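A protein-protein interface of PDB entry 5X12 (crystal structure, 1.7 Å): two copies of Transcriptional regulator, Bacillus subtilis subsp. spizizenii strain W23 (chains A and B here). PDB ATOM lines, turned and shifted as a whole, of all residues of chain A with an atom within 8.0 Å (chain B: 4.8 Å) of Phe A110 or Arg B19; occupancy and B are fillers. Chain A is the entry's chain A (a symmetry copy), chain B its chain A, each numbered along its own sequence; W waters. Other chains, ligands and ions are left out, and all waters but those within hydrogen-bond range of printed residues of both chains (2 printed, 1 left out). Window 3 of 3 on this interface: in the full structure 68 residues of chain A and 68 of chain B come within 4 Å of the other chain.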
ATOM      1  N   GLU A 103     -14.373 -33.676 -10.095  1.00  0.00           N
ATOM      2  CA  GLU A 103     -15.325 -32.777 -10.681  1.00  0.00           C
ATOM      3  C   GLU A 103     -16.409 -32.383  -9.695  1.00  0.00           C
ATOM      4  O   GLU A 103     -16.874 -31.247  -9.680  1.00  0.00           O
ATOM      5  CB  GLU A 103     -15.998 -33.376 -11.867  1.00  0.00           C
ATOM      6  CG  GLU A 103     -16.674 -32.366 -12.733  1.00  0.00           C
ATOM      7  CD  GLU A 103     -16.993 -32.938 -14.123  1.00  0.00           C
ATOM      8  OE1 GLU A 103     -16.570 -34.078 -14.422  1.00  0.00           O
ATOM      9  OE2 GLU A 103     -17.638 -32.242 -14.908  1.00  0.00           O
ATOM     10  N   PHE A 104     -16.842 -33.346  -8.871  1.00  0.00           N
ATOM     11  CA  PHE A 104     -17.810 -32.988  -7.837  1.00  0.00           C
ATOM     12  C   PHE A 104     -17.282 -31.864  -6.913  1.00  0.00           C
ATOM     13  O   PHE A 104     -18.037 -31.000  -6.474  1.00  0.00           O
ATOM     14  CB  PHE A 104     -18.193 -34.214  -6.974  1.00  0.00           C
ATOM     15  CG  PHE A 104     -19.138 -33.873  -5.865  1.00  0.00           C
ATOM     16  CD1 PHE A 104     -20.477 -33.768  -6.120  1.00  0.00           C
ATOM     17  CD2 PHE A 104     -18.688 -33.693  -4.577  1.00  0.00           C
ATOM     18  CE1 PHE A 104     -21.369 -33.416  -5.110  1.00  0.00           C
ATOM     19  CE2 PHE A 104     -19.566 -33.349  -3.593  1.00  0.00           C
ATOM     20  CZ  PHE A 104     -20.907 -33.201  -3.877  1.00  0.00           C
ATOM     21  N   MET A 105     -16.014 -31.909  -6.542  1.00  0.00           N
ATOM     22  CA  MET A 105     -15.432 -30.889  -5.691  1.00  0.00           C
ATOM     23  C   MET A 105     -15.325 -29.539  -6.347  1.00  0.00           C
ATOM     24  O   MET A 105     -15.415 -28.499  -5.674  1.00  0.00           O
ATOM     25  CB  MET A 105     -14.067 -31.324  -5.137  1.00  0.00           C
ATOM     26  CG  MET A 105     -14.226 -32.543  -4.109  1.00  0.00           C
ATOM     27  SD  MET A 105     -15.446 -32.209  -2.822  1.00  0.00           S
ATOM     28  CE  MET A 105     -14.716 -30.680  -2.178  1.00  0.00           C
ATOM     29  N   LEU A 106     -15.169 -29.508  -7.675  1.00  0.00           N
ATOM     30  CA  LEU A 106     -15.285 -28.232  -8.368  1.00  0.00           C
ATOM     31  C   LEU A 106     -16.696 -27.667  -8.256  1.00  0.00           C
ATOM     32  O   LEU A 106     -16.861 -26.475  -8.050  1.00  0.00           O
ATOM     33  CB  LEU A 106     -14.815 -28.323  -9.837  1.00  0.00           C
ATOM     34  CG  LEU A 106     -14.639 -27.039 -10.593  1.00  0.00           C
ATOM     35  CD1 LEU A 106     -13.403 -26.255 -10.038  1.00  0.00           C
ATOM     36  CD2 LEU A 106     -14.452 -27.340 -12.078  1.00  0.00           C
ATOM     37  N   LYS A 107     -17.727 -28.535  -8.337  1.00  0.00           N
ATOM     38  CA  LYS A 107     -19.077 -28.102  -8.122  1.00  0.00           C
ATOM     39  C   LYS A 107     -19.243 -27.557  -6.712  1.00  0.00           C
ATOM     40  O   LYS A 107     -19.843 -26.504  -6.526  1.00  0.00           O
ATOM     41  CB  LYS A 107     -20.060 -29.247  -8.353  1.00  0.00           C
ATOM     42  CG  LYS A 107     -20.095 -29.714  -9.789  1.00  0.00           C
ATOM     43  CD  LYS A 107     -21.192 -30.767  -9.953  1.00  0.00           C
ATOM     44  CE  LYS A 107     -21.229 -31.366 -11.312  1.00  0.00           C
ATOM     45  NZ  LYS A 107     -22.598 -32.101 -11.391  1.00  0.00           N
ATOM     46  N   ALA A 108     -18.667 -28.261  -5.716  1.00  0.00           N
ATOM     47  CA  ALA A 108     -18.765 -27.825  -4.348  1.00  0.00           C
ATOM     48  C   ALA A 108     -18.160 -26.409  -4.152  1.00  0.00           C
ATOM     49  O   ALA A 108     -18.703 -25.561  -3.422  1.00  0.00           O
ATOM     50  CB  ALA A 108     -18.052 -28.864  -3.426  1.00  0.00           C
ATOM     51  N   TYR A 109     -17.025 -26.171  -4.786  1.00  0.00           N
ATOM     52  CA  TYR A 109     -16.355 -24.881  -4.746  1.00  0.00           C
ATOM     53  C   TYR A 109     -17.307 -23.730  -5.220  1.00  0.00           C
ATOM     54  O   TYR A 109     -17.227 -22.608  -4.693  1.00  0.00           O
ATOM     55  CB  TYR A 109     -15.100 -24.930  -5.604  1.00  0.00           C
ATOM     56  CG  TYR A 109     -14.219 -23.724  -5.566  1.00  0.00           C
ATOM     57  CD1 TYR A 109     -13.558 -23.352  -4.388  1.00  0.00           C
ATOM     58  CD2 TYR A 109     -14.023 -22.949  -6.688  1.00  0.00           C
ATOM     59  CE1 TYR A 109     -12.750 -22.248  -4.355  1.00  0.00           C
ATOM     60  CE2 TYR A 109     -13.209 -21.837  -6.669  1.00  0.00           C
ATOM     61  CZ  TYR A 109     -12.566 -21.488  -5.496  1.00  0.00           C
ATOM     62  OH  TYR A 109     -11.761 -20.364  -5.502  1.00  0.00           O
ATOM     63  N   PHE A 110     -18.191 -24.040  -6.182  1.00  0.00           N
ATOM     64  CA  PHE A 110     -19.125 -23.071  -6.770  1.00  0.00           C
ATOM     65  C   PHE A 110     -20.535 -23.193  -6.225  1.00  0.00           C
ATOM     66  O   PHE A 110     -21.521 -22.724  -6.835  1.00  0.00           O
ATOM     67  CB  PHE A 110     -19.085 -23.292  -8.327  1.00  0.00           C
ATOM     68  CG  PHE A 110     -17.767 -22.996  -8.930  1.00  0.00           C
ATOM     69  CD1 PHE A 110     -17.062 -21.817  -8.629  1.00  0.00           C
ATOM     70  CD2 PHE A 110     -17.206 -23.855  -9.876  1.00  0.00           C
ATOM     71  CE1 PHE A 110     -15.863 -21.538  -9.195  1.00  0.00           C
ATOM     72  CE2 PHE A 110     -15.988 -23.551 -10.472  1.00  0.00           C
ATOM     73  CZ  PHE A 110     -15.312 -22.389 -10.121  1.00  0.00           C
ATOM     74  N   ILE A 111     -20.645 -23.785  -5.029  1.00  0.00           N
ATOM     75  CA  ILE A 111     -21.949 -24.012  -4.385  1.00  0.00           C
ATOM     76  C   ILE A 111     -22.815 -22.758  -4.217  1.00  0.00           C
ATOM     77  O   ILE A 111     -24.058 -22.844  -4.111  1.00  0.00           O
ATOM     78  CB  ILE A 111     -21.770 -24.710  -3.000  1.00  0.00           C
ATOM     79  CG1 ILE A 111     -23.100 -25.310  -2.507  1.00  0.00           C
ATOM     80  CG2 ILE A 111     -21.126 -23.732  -1.958  1.00  0.00           C
ATOM     81  CD1 ILE A 111     -22.939 -26.283  -1.305  1.00  0.00           C
ATOM     82  N   SER A 112     -22.214 -21.578  -4.194  1.00  0.00           N
ATOM     83  CA  SER A 112     -22.998 -20.343  -4.017  1.00  0.00           C
ATOM     84  C   SER A 112     -23.999 -20.150  -5.175  1.00  0.00           C
ATOM     85  O   SER A 112     -24.958 -19.382  -5.013  1.00  0.00           O
ATOM     86  CB  SER A 112     -22.122 -19.085  -3.954  1.00  0.00           C
ATOM     87  OG  SER A 112     -21.430 -18.859  -5.200  1.00  0.00           O
ATOM     88  N   SER A 113     -23.778 -20.822  -6.319  1.00  0.00           N
ATOM     89  CA  SER A 113     -24.684 -20.764  -7.445  1.00  0.00           C
ATOM     90  C   SER A 113     -25.929 -21.655  -7.309  1.00  0.00           C
ATOM     91  O   SER A 113     -26.814 -21.606  -8.169  1.00  0.00           O
ATOM     92  CB  SER A 113     -23.947 -21.091  -8.737  1.00  0.00           C
ATOM     93  OG  SER A 113     -23.111 -20.012  -9.133  1.00  0.00           O
ATOM     94  N   LEU A 114     -26.007 -22.442  -6.222  1.00  0.00           N
ATOM     95  CA  LEU A 114     -27.139 -23.345  -5.932  1.00  0.00           C
ATOM     96  C   LEU A 114     -27.939 -22.880  -4.720  1.00  0.00           C
ATOM     97  O   LEU A 114     -27.382 -22.333  -3.751  1.00  0.00           O
ATOM     98  CB  LEU A 114     -26.615 -24.769  -5.676  1.00  0.00           C
ATOM     99  CG  LEU A 114     -25.911 -25.411  -6.856  1.00  0.00           C
ATOM    100  CD1 LEU A 114     -25.485 -26.843  -6.442  1.00  0.00           C
ATOM    101  CD2 LEU A 114     -26.710 -25.400  -8.157  1.00  0.00           C
ATOM    102  N   LEU A 122     -27.829 -32.164  -4.774  1.00  0.00           N
ATOM    103  CA  LEU A 122     -26.503 -32.485  -5.366  1.00  0.00           C
ATOM    104  C   LEU A 122     -25.661 -33.359  -4.442  1.00  0.00           C
ATOM    105  O   LEU A 122     -25.160 -34.408  -4.837  1.00  0.00           O
ATOM    106  CB  LEU A 122     -25.780 -31.220  -5.756  1.00  0.00           C
ATOM    107  CG  LEU A 122     -24.326 -31.389  -6.242  1.00  0.00           C
ATOM    108  CD1 LEU A 122     -24.352 -32.216  -7.491  1.00  0.00           C
ATOM    109  CD2 LEU A 122     -23.594 -30.000  -6.332  1.00  0.00           C
ATOM    110  N   TYR B  12     -15.511 -25.140 -16.846  1.00  0.00           N
ATOM    111  CA  TYR B  12     -16.437 -24.875 -15.712  1.00  0.00           C
ATOM    112  C   TYR B  12     -15.740 -24.174 -14.593  1.00  0.00           C
ATOM    113  O   TYR B  12     -16.370 -23.435 -13.815  1.00  0.00           O
ATOM    114  CB  TYR B  12     -17.236 -26.137 -15.342  1.00  0.00           C
ATOM    115  CG  TYR B  12     -18.139 -26.572 -16.460  1.00  0.00           C
ATOM    116  CD1 TYR B  12     -19.317 -25.867 -16.720  1.00  0.00           C
ATOM    117  CD2 TYR B  12     -17.797 -27.605 -17.332  1.00  0.00           C
ATOM    118  CE1 TYR B  12     -20.099 -26.162 -17.762  1.00  0.00           C
ATOM    119  CE2 TYR B  12     -18.605 -27.928 -18.416  1.00  0.00           C
ATOM    120  CZ  TYR B  12     -19.772 -27.203 -18.622  1.00  0.00           C
ATOM    121  OH  TYR B  12     -20.577 -27.534 -19.693  1.00  0.00           O
ATOM    122  N   ALA B  13     -14.430 -24.373 -14.484  1.00  0.00           N
ATOM    123  CA  ALA B  13     -13.639 -23.599 -13.550  1.00  0.00           C
ATOM    124  C   ALA B  13     -13.681 -22.112 -13.909  1.00  0.00           C
ATOM    125  O   ALA B  13     -13.943 -21.282 -13.053  1.00  0.00           O
ATOM    126  CB  ALA B  13     -12.234 -24.154 -13.461  1.00  0.00           C
ATOM    127  N   LEU B  15     -16.094 -20.480 -15.863  1.00  0.00           N
ATOM    128  CA  LEU B  15     -17.461 -20.006 -15.761  1.00  0.00           C
ATOM    129  C   LEU B  15     -17.765 -19.832 -14.269  1.00  0.00           C
ATOM    130  O   LEU B  15     -18.352 -18.841 -13.866  1.00  0.00           O
ATOM    131  CB  LEU B  15     -18.437 -20.956 -16.434  1.00  0.00           C
ATOM    132  CG  LEU B  15     -18.314 -21.202 -17.939  1.00  0.00           C
ATOM    133  CD1 LEU B  15     -19.319 -22.221 -18.421  1.00  0.00           C
ATOM    134  CD2 LEU B  15     -18.541 -19.899 -18.677  1.00  0.00           C
ATOM    135  N   GLY B  16     -17.378 -20.799 -13.428  1.00  0.00           N
ATOM    136  CA  GLY B  16     -17.710 -20.724 -12.039  1.00  0.00           C
ATOM    137  C   GLY B  16     -17.022 -19.558 -11.340  1.00  0.00           C
ATOM    138  O   GLY B  16     -17.601 -18.897 -10.480  1.00  0.00           O
ATOM    139  N   LEU B  17     -15.777 -19.278 -11.731  1.00  0.00           N
ATOM    140  CA  LEU B  17     -15.048 -18.179 -11.135  1.00  0.00           C
ATOM    141  C   LEU B  17     -15.791 -16.853 -11.336  1.00  0.00           C
ATOM    142  O   LEU B  17     -15.692 -15.978 -10.491  1.00  0.00           O
ATOM    143  CB  LEU B  17     -13.626 -18.073 -11.687  1.00  0.00           C
ATOM    144  CG  LEU B  17     -12.584 -19.007 -11.089  1.00  0.00           C
ATOM    145  CD1 LEU B  17     -11.244 -18.834 -11.853  1.00  0.00           C
ATOM    146  CD2 LEU B  17     -12.422 -18.794  -9.528  1.00  0.00           C
ATOM    147  N   LEU B  18     -16.556 -16.744 -12.431  1.00  0.00           N
ATOM    148  CA  LEU B  18     -17.253 -15.513 -12.774  1.00  0.00           C
ATOM    149  C   LEU B  18     -18.688 -15.424 -12.209  1.00  0.00           C
ATOM    150  O   LEU B  18     -19.385 -14.426 -12.406  1.00  0.00           O
ATOM    151  CB  LEU B  18     -17.285 -15.316 -14.284  1.00  0.00           C
ATOM    152  CG  LEU B  18     -15.963 -15.231 -15.025  1.00  0.00           C
ATOM    153  CD1 LEU B  18     -16.145 -15.266 -16.572  1.00  0.00           C
ATOM    154  CD2 LEU B  18     -15.274 -13.949 -14.600  1.00  0.00           C
ATOM    155  N   ARG B  19     -19.103 -16.419 -11.443  1.00  0.00           N
ATOM    156  CA  ARG B  19     -20.491 -16.533 -10.968  1.00  0.00           C
ATOM    157  C   ARG B  19     -20.931 -15.389 -10.058  1.00  0.00           C
ATOM    158  O   ARG B  19     -22.125 -15.120  -9.955  1.00  0.00           O
ATOM    159  CB  ARG B  19     -20.673 -17.866 -10.244  1.00  0.00           C
ATOM    160  CG  ARG B  19     -20.089 -17.923  -8.867  1.00  0.00           C
ATOM    161  CD  ARG B  19     -19.866 -19.362  -8.351  1.00  0.00           C
ATOM    162  NE  ARG B  19     -19.345 -19.314  -6.999  1.00  0.00           N
ATOM    163  CZ  ARG B  19     -18.116 -18.877  -6.684  1.00  0.00           C
ATOM    164  NH1 ARG B  19     -17.256 -18.506  -7.631  1.00  0.00           N
ATOM    165  NH2 ARG B  19     -17.761 -18.796  -5.424  1.00  0.00           N
ATOM    166  N   LYS B  20     -19.995 -14.742  -9.381  1.00  0.00           N
ATOM    167  CA  LYS B  20     -20.359 -13.674  -8.456  1.00  0.00           C
ATOM    168  C   LYS B  20     -20.133 -12.280  -9.016  1.00  0.00           C
ATOM    169  O   LYS B  20     -20.377 -11.291  -8.325  1.00  0.00           O
ATOM    170  CB  LYS B  20     -19.613 -13.841  -7.144  1.00  0.00           C
ATOM    171  CG  LYS B  20     -20.295 -14.827  -6.212  1.00  0.00           C
ATOM    172  CD  LYS B  20     -19.575 -14.926  -4.877  1.00  0.00           C
ATOM    173  CE  LYS B  20     -20.173 -16.004  -3.982  1.00  0.00           C
ATOM    174  NZ  LYS B  20     -21.147 -15.518  -2.953  1.00  0.00           N
ATOM    175  N   GLY B  21     -19.694 -12.197 -10.258  1.00  0.00           N
ATOM    176  CA  GLY B  21     -19.447 -10.912 -10.890  1.00  0.00           C
ATOM    177  C   GLY B  21     -18.145 -10.878 -11.642  1.00  0.00           C
ATOM    178  O   GLY B  21     -17.422 -11.888 -11.706  1.00  0.00           O
ATOM    179  N   LEU B  78     -20.187 -13.381 -16.946  1.00  0.00           N
ATOM    180  CA  LEU B  78     -21.070 -14.401 -17.554  1.00  0.00           C
ATOM    181  C   LEU B  78     -22.200 -13.736 -18.309  1.00  0.00           C
ATOM    182  O   LEU B  78     -22.758 -12.734 -17.866  1.00  0.00           O
ATOM    183  CB  LEU B  78     -21.697 -15.329 -16.531  1.00  0.00           C
ATOM    184  CG  LEU B  78     -20.776 -16.288 -15.820  1.00  0.00           C
ATOM    185  CD1 LEU B  78     -21.622 -17.045 -14.676  1.00  0.00           C
ATOM    186  CD2 LEU B  78     -20.080 -17.303 -16.722  1.00  0.00           C
ATOM    187  N   LEU B  86     -23.324 -23.087 -16.748  1.00  0.00           N
ATOM    188  CA  LEU B  86     -22.809 -23.418 -15.402  1.00  0.00           C
ATOM    189  C   LEU B  86     -23.863 -24.129 -14.544  1.00  0.00           C
ATOM    190  O   LEU B  86     -23.596 -25.177 -13.963  1.00  0.00           O
ATOM    191  CB  LEU B  86     -22.308 -22.134 -14.751  1.00  0.00           C
ATOM    192  CG  LEU B  86     -21.840 -22.267 -13.312  1.00  0.00           C
ATOM    193  CD1 LEU B  86     -20.576 -23.118 -13.315  1.00  0.00           C
ATOM    194  CD2 LEU B  86     -21.628 -20.816 -12.721  1.00  0.00           C
ATOM    195  N   TRP B  89     -24.527 -27.802 -15.669  1.00  0.00           N
ATOM    196  CA  TRP B  89     -23.411 -28.663 -15.254  1.00  0.00           C
ATOM    197  C   TRP B  89     -23.476 -28.938 -13.734  1.00  0.00           C
ATOM    198  O   TRP B  89     -23.273 -30.069 -13.271  1.00  0.00           O
ATOM    199  CB  TRP B  89     -22.108 -27.994 -15.602  1.00  0.00           C
ATOM    200  CG  TRP B  89     -20.876 -28.574 -15.018  1.00  0.00           C
ATOM    201  CD1 TRP B  89     -20.207 -29.696 -15.435  1.00  0.00           C
ATOM    202  CD2 TRP B  89     -20.100 -28.020 -13.952  1.00  0.00           C
ATOM    203  NE1 TRP B  89     -19.104 -29.892 -14.650  1.00  0.00           N
ATOM    204  CE2 TRP B  89     -19.021 -28.870 -13.744  1.00  0.00           C
ATOM    205  CE3 TRP B  89     -20.254 -26.887 -13.126  1.00  0.00           C
ATOM    206  CZ2 TRP B  89     -18.063 -28.626 -12.761  1.00  0.00           C
ATOM    207  CZ3 TRP B  89     -19.314 -26.643 -12.168  1.00  0.00           C
ATOM    208  CH2 TRP B  89     -18.223 -27.487 -12.011  1.00  0.00           C
ATOM    209  N   LEU B  90     -23.762 -27.891 -12.954  1.00  0.00           N
ATOM    210  CA  LEU B  90     -23.797 -28.055 -11.487  1.00  0.00           C
ATOM    211  C   LEU B  90     -24.863 -29.081 -11.095  1.00  0.00           C
ATOM    212  O   LEU B  90     -24.650 -29.943 -10.231  1.00  0.00           O
ATOM    213  CB  LEU B  90     -24.073 -26.713 -10.761  1.00  0.00           C
ATOM    214  CG  LEU B  90     -22.929 -25.702 -10.687  1.00  0.00           C
ATOM    215  CD1 LEU B  90     -23.479 -24.345 -10.308  1.00  0.00           C
ATOM    216  CD2 LEU B  90     -21.826 -26.169  -9.713  1.00  0.00           C
HETATM  217  O   HOH W   1     -21.669 -32.757 -14.677  1.00  0.00           O
HETATM  218  O   HOH W   2     -15.578 -20.400  -4.022  1.00  0.00           O
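The guanidinium group of Arg B19 lies within hydrogen-bond range of the side-chain hydroxyl of Ser A112 (2.8 Å). The side-chain carboxylate of Glu A103 sits at hydrogen-bond distance from the indole nitrogen of Trp B89 (2.8 Å). The backbone carbonyl oxygen (O) of Trp B89 sits at hydrogen-bond distance from the side-chain amino group (NZ) of Lys A107 (2.8 Å). O of Leu B90 lies within hydrogen-bond range of NZ of Lys A107, 3.2 Å away.
No position is printed for both chains. Of the 18 pairs that touch across the chains among the printed residues, none has its exchanged pair printed and touching as well.
Among the printed residues, merely in contact across the chains: Leu A106 with Ala B13 (3.8 Å), Leu A106 with Trp B89 (3.8 Å), Tyr A109 with Arg B19 (3.9 Å), Phe A110 with Tyr B12 (3.4 Å), Phe A110 with Ala B13 (3.4 Å), Phe A110 with Gly B16 (3.1 Å), Phe A110 with Leu B17 (3.4 Å), Phe A110 with Arg B19 (3.5 Å), Ser A112 with Lys B20 (3.3 Å), Ser A113 with Arg B19 (3.4 Å), Ser A113 with Leu B86 (3.96 Å), Ser A113 with Leu B90 (3.6 Å), Leu A114 with Leu B90 (3.9 Å) and Leu A122 with Leu B90 (3.6 Å).
Water W2 lies within hydrogen-bond range of the backbone carbonyl oxygen of Tyr A109 and the guanidinium group of Arg B19. Water W1 lies within hydrogen-bond range of the backbone carbonyl oxygen (O) of Trp B89 and the side-chain amino group (NZ) of Lys A107.
O of Gly B16 lies within hydrogen-bond range of NH1 of Arg B19, at 2.9 Å.
Of the printed residues of chain B, Tyr A109 touches Arg B19 (3.9 Å). Of chain B, only Tyr B12 (3.4 Å), Ala B13 (3.4 Å), Gly B16 (3.1 Å), Leu B17 (3.4 Å) and Arg B19 (3.5 Å) come within 4 Å of Phe A110. Of the printed residues of chain B, Ser A113 touches Arg B19 (3.4 Å), Leu B86 (3.96 Å) and Leu B90 (3.6 Å). Of the printed residues of chain A, Gly B16 touches Phe A110 (3.1 Å). Arg B19 touches just these residues of chain A: Tyr A109 (3.9 Å), Phe A110 (3.5 Å), Ser A112 (2.8 Å) and Ser A113 (3.4 Å). The nearest residue of chain A that does not touch Arg B19 is Ile A111 (5.1 Å). The nearest printed residue of chain B that does not touch Leu A114 is Leu B86 (6.6 Å).
Hydrophobic or aromatic side chains of chain B within 4 Å of the printed part of chain A: Leu B86, Trp B89 and Leu B90. Of the 13 printed residues of chain A, 9 touch a printed residue of chain B. Along chain A the printed residues that touch a printed residue of chain B span positions 103 to 122. Among the printed residues, 18 pairs touch across the chains. Among the printed residues, no Asp or Glu carboxylate lies within 4 Å of a Lys or Arg side-chain nitrogen of the other chain.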
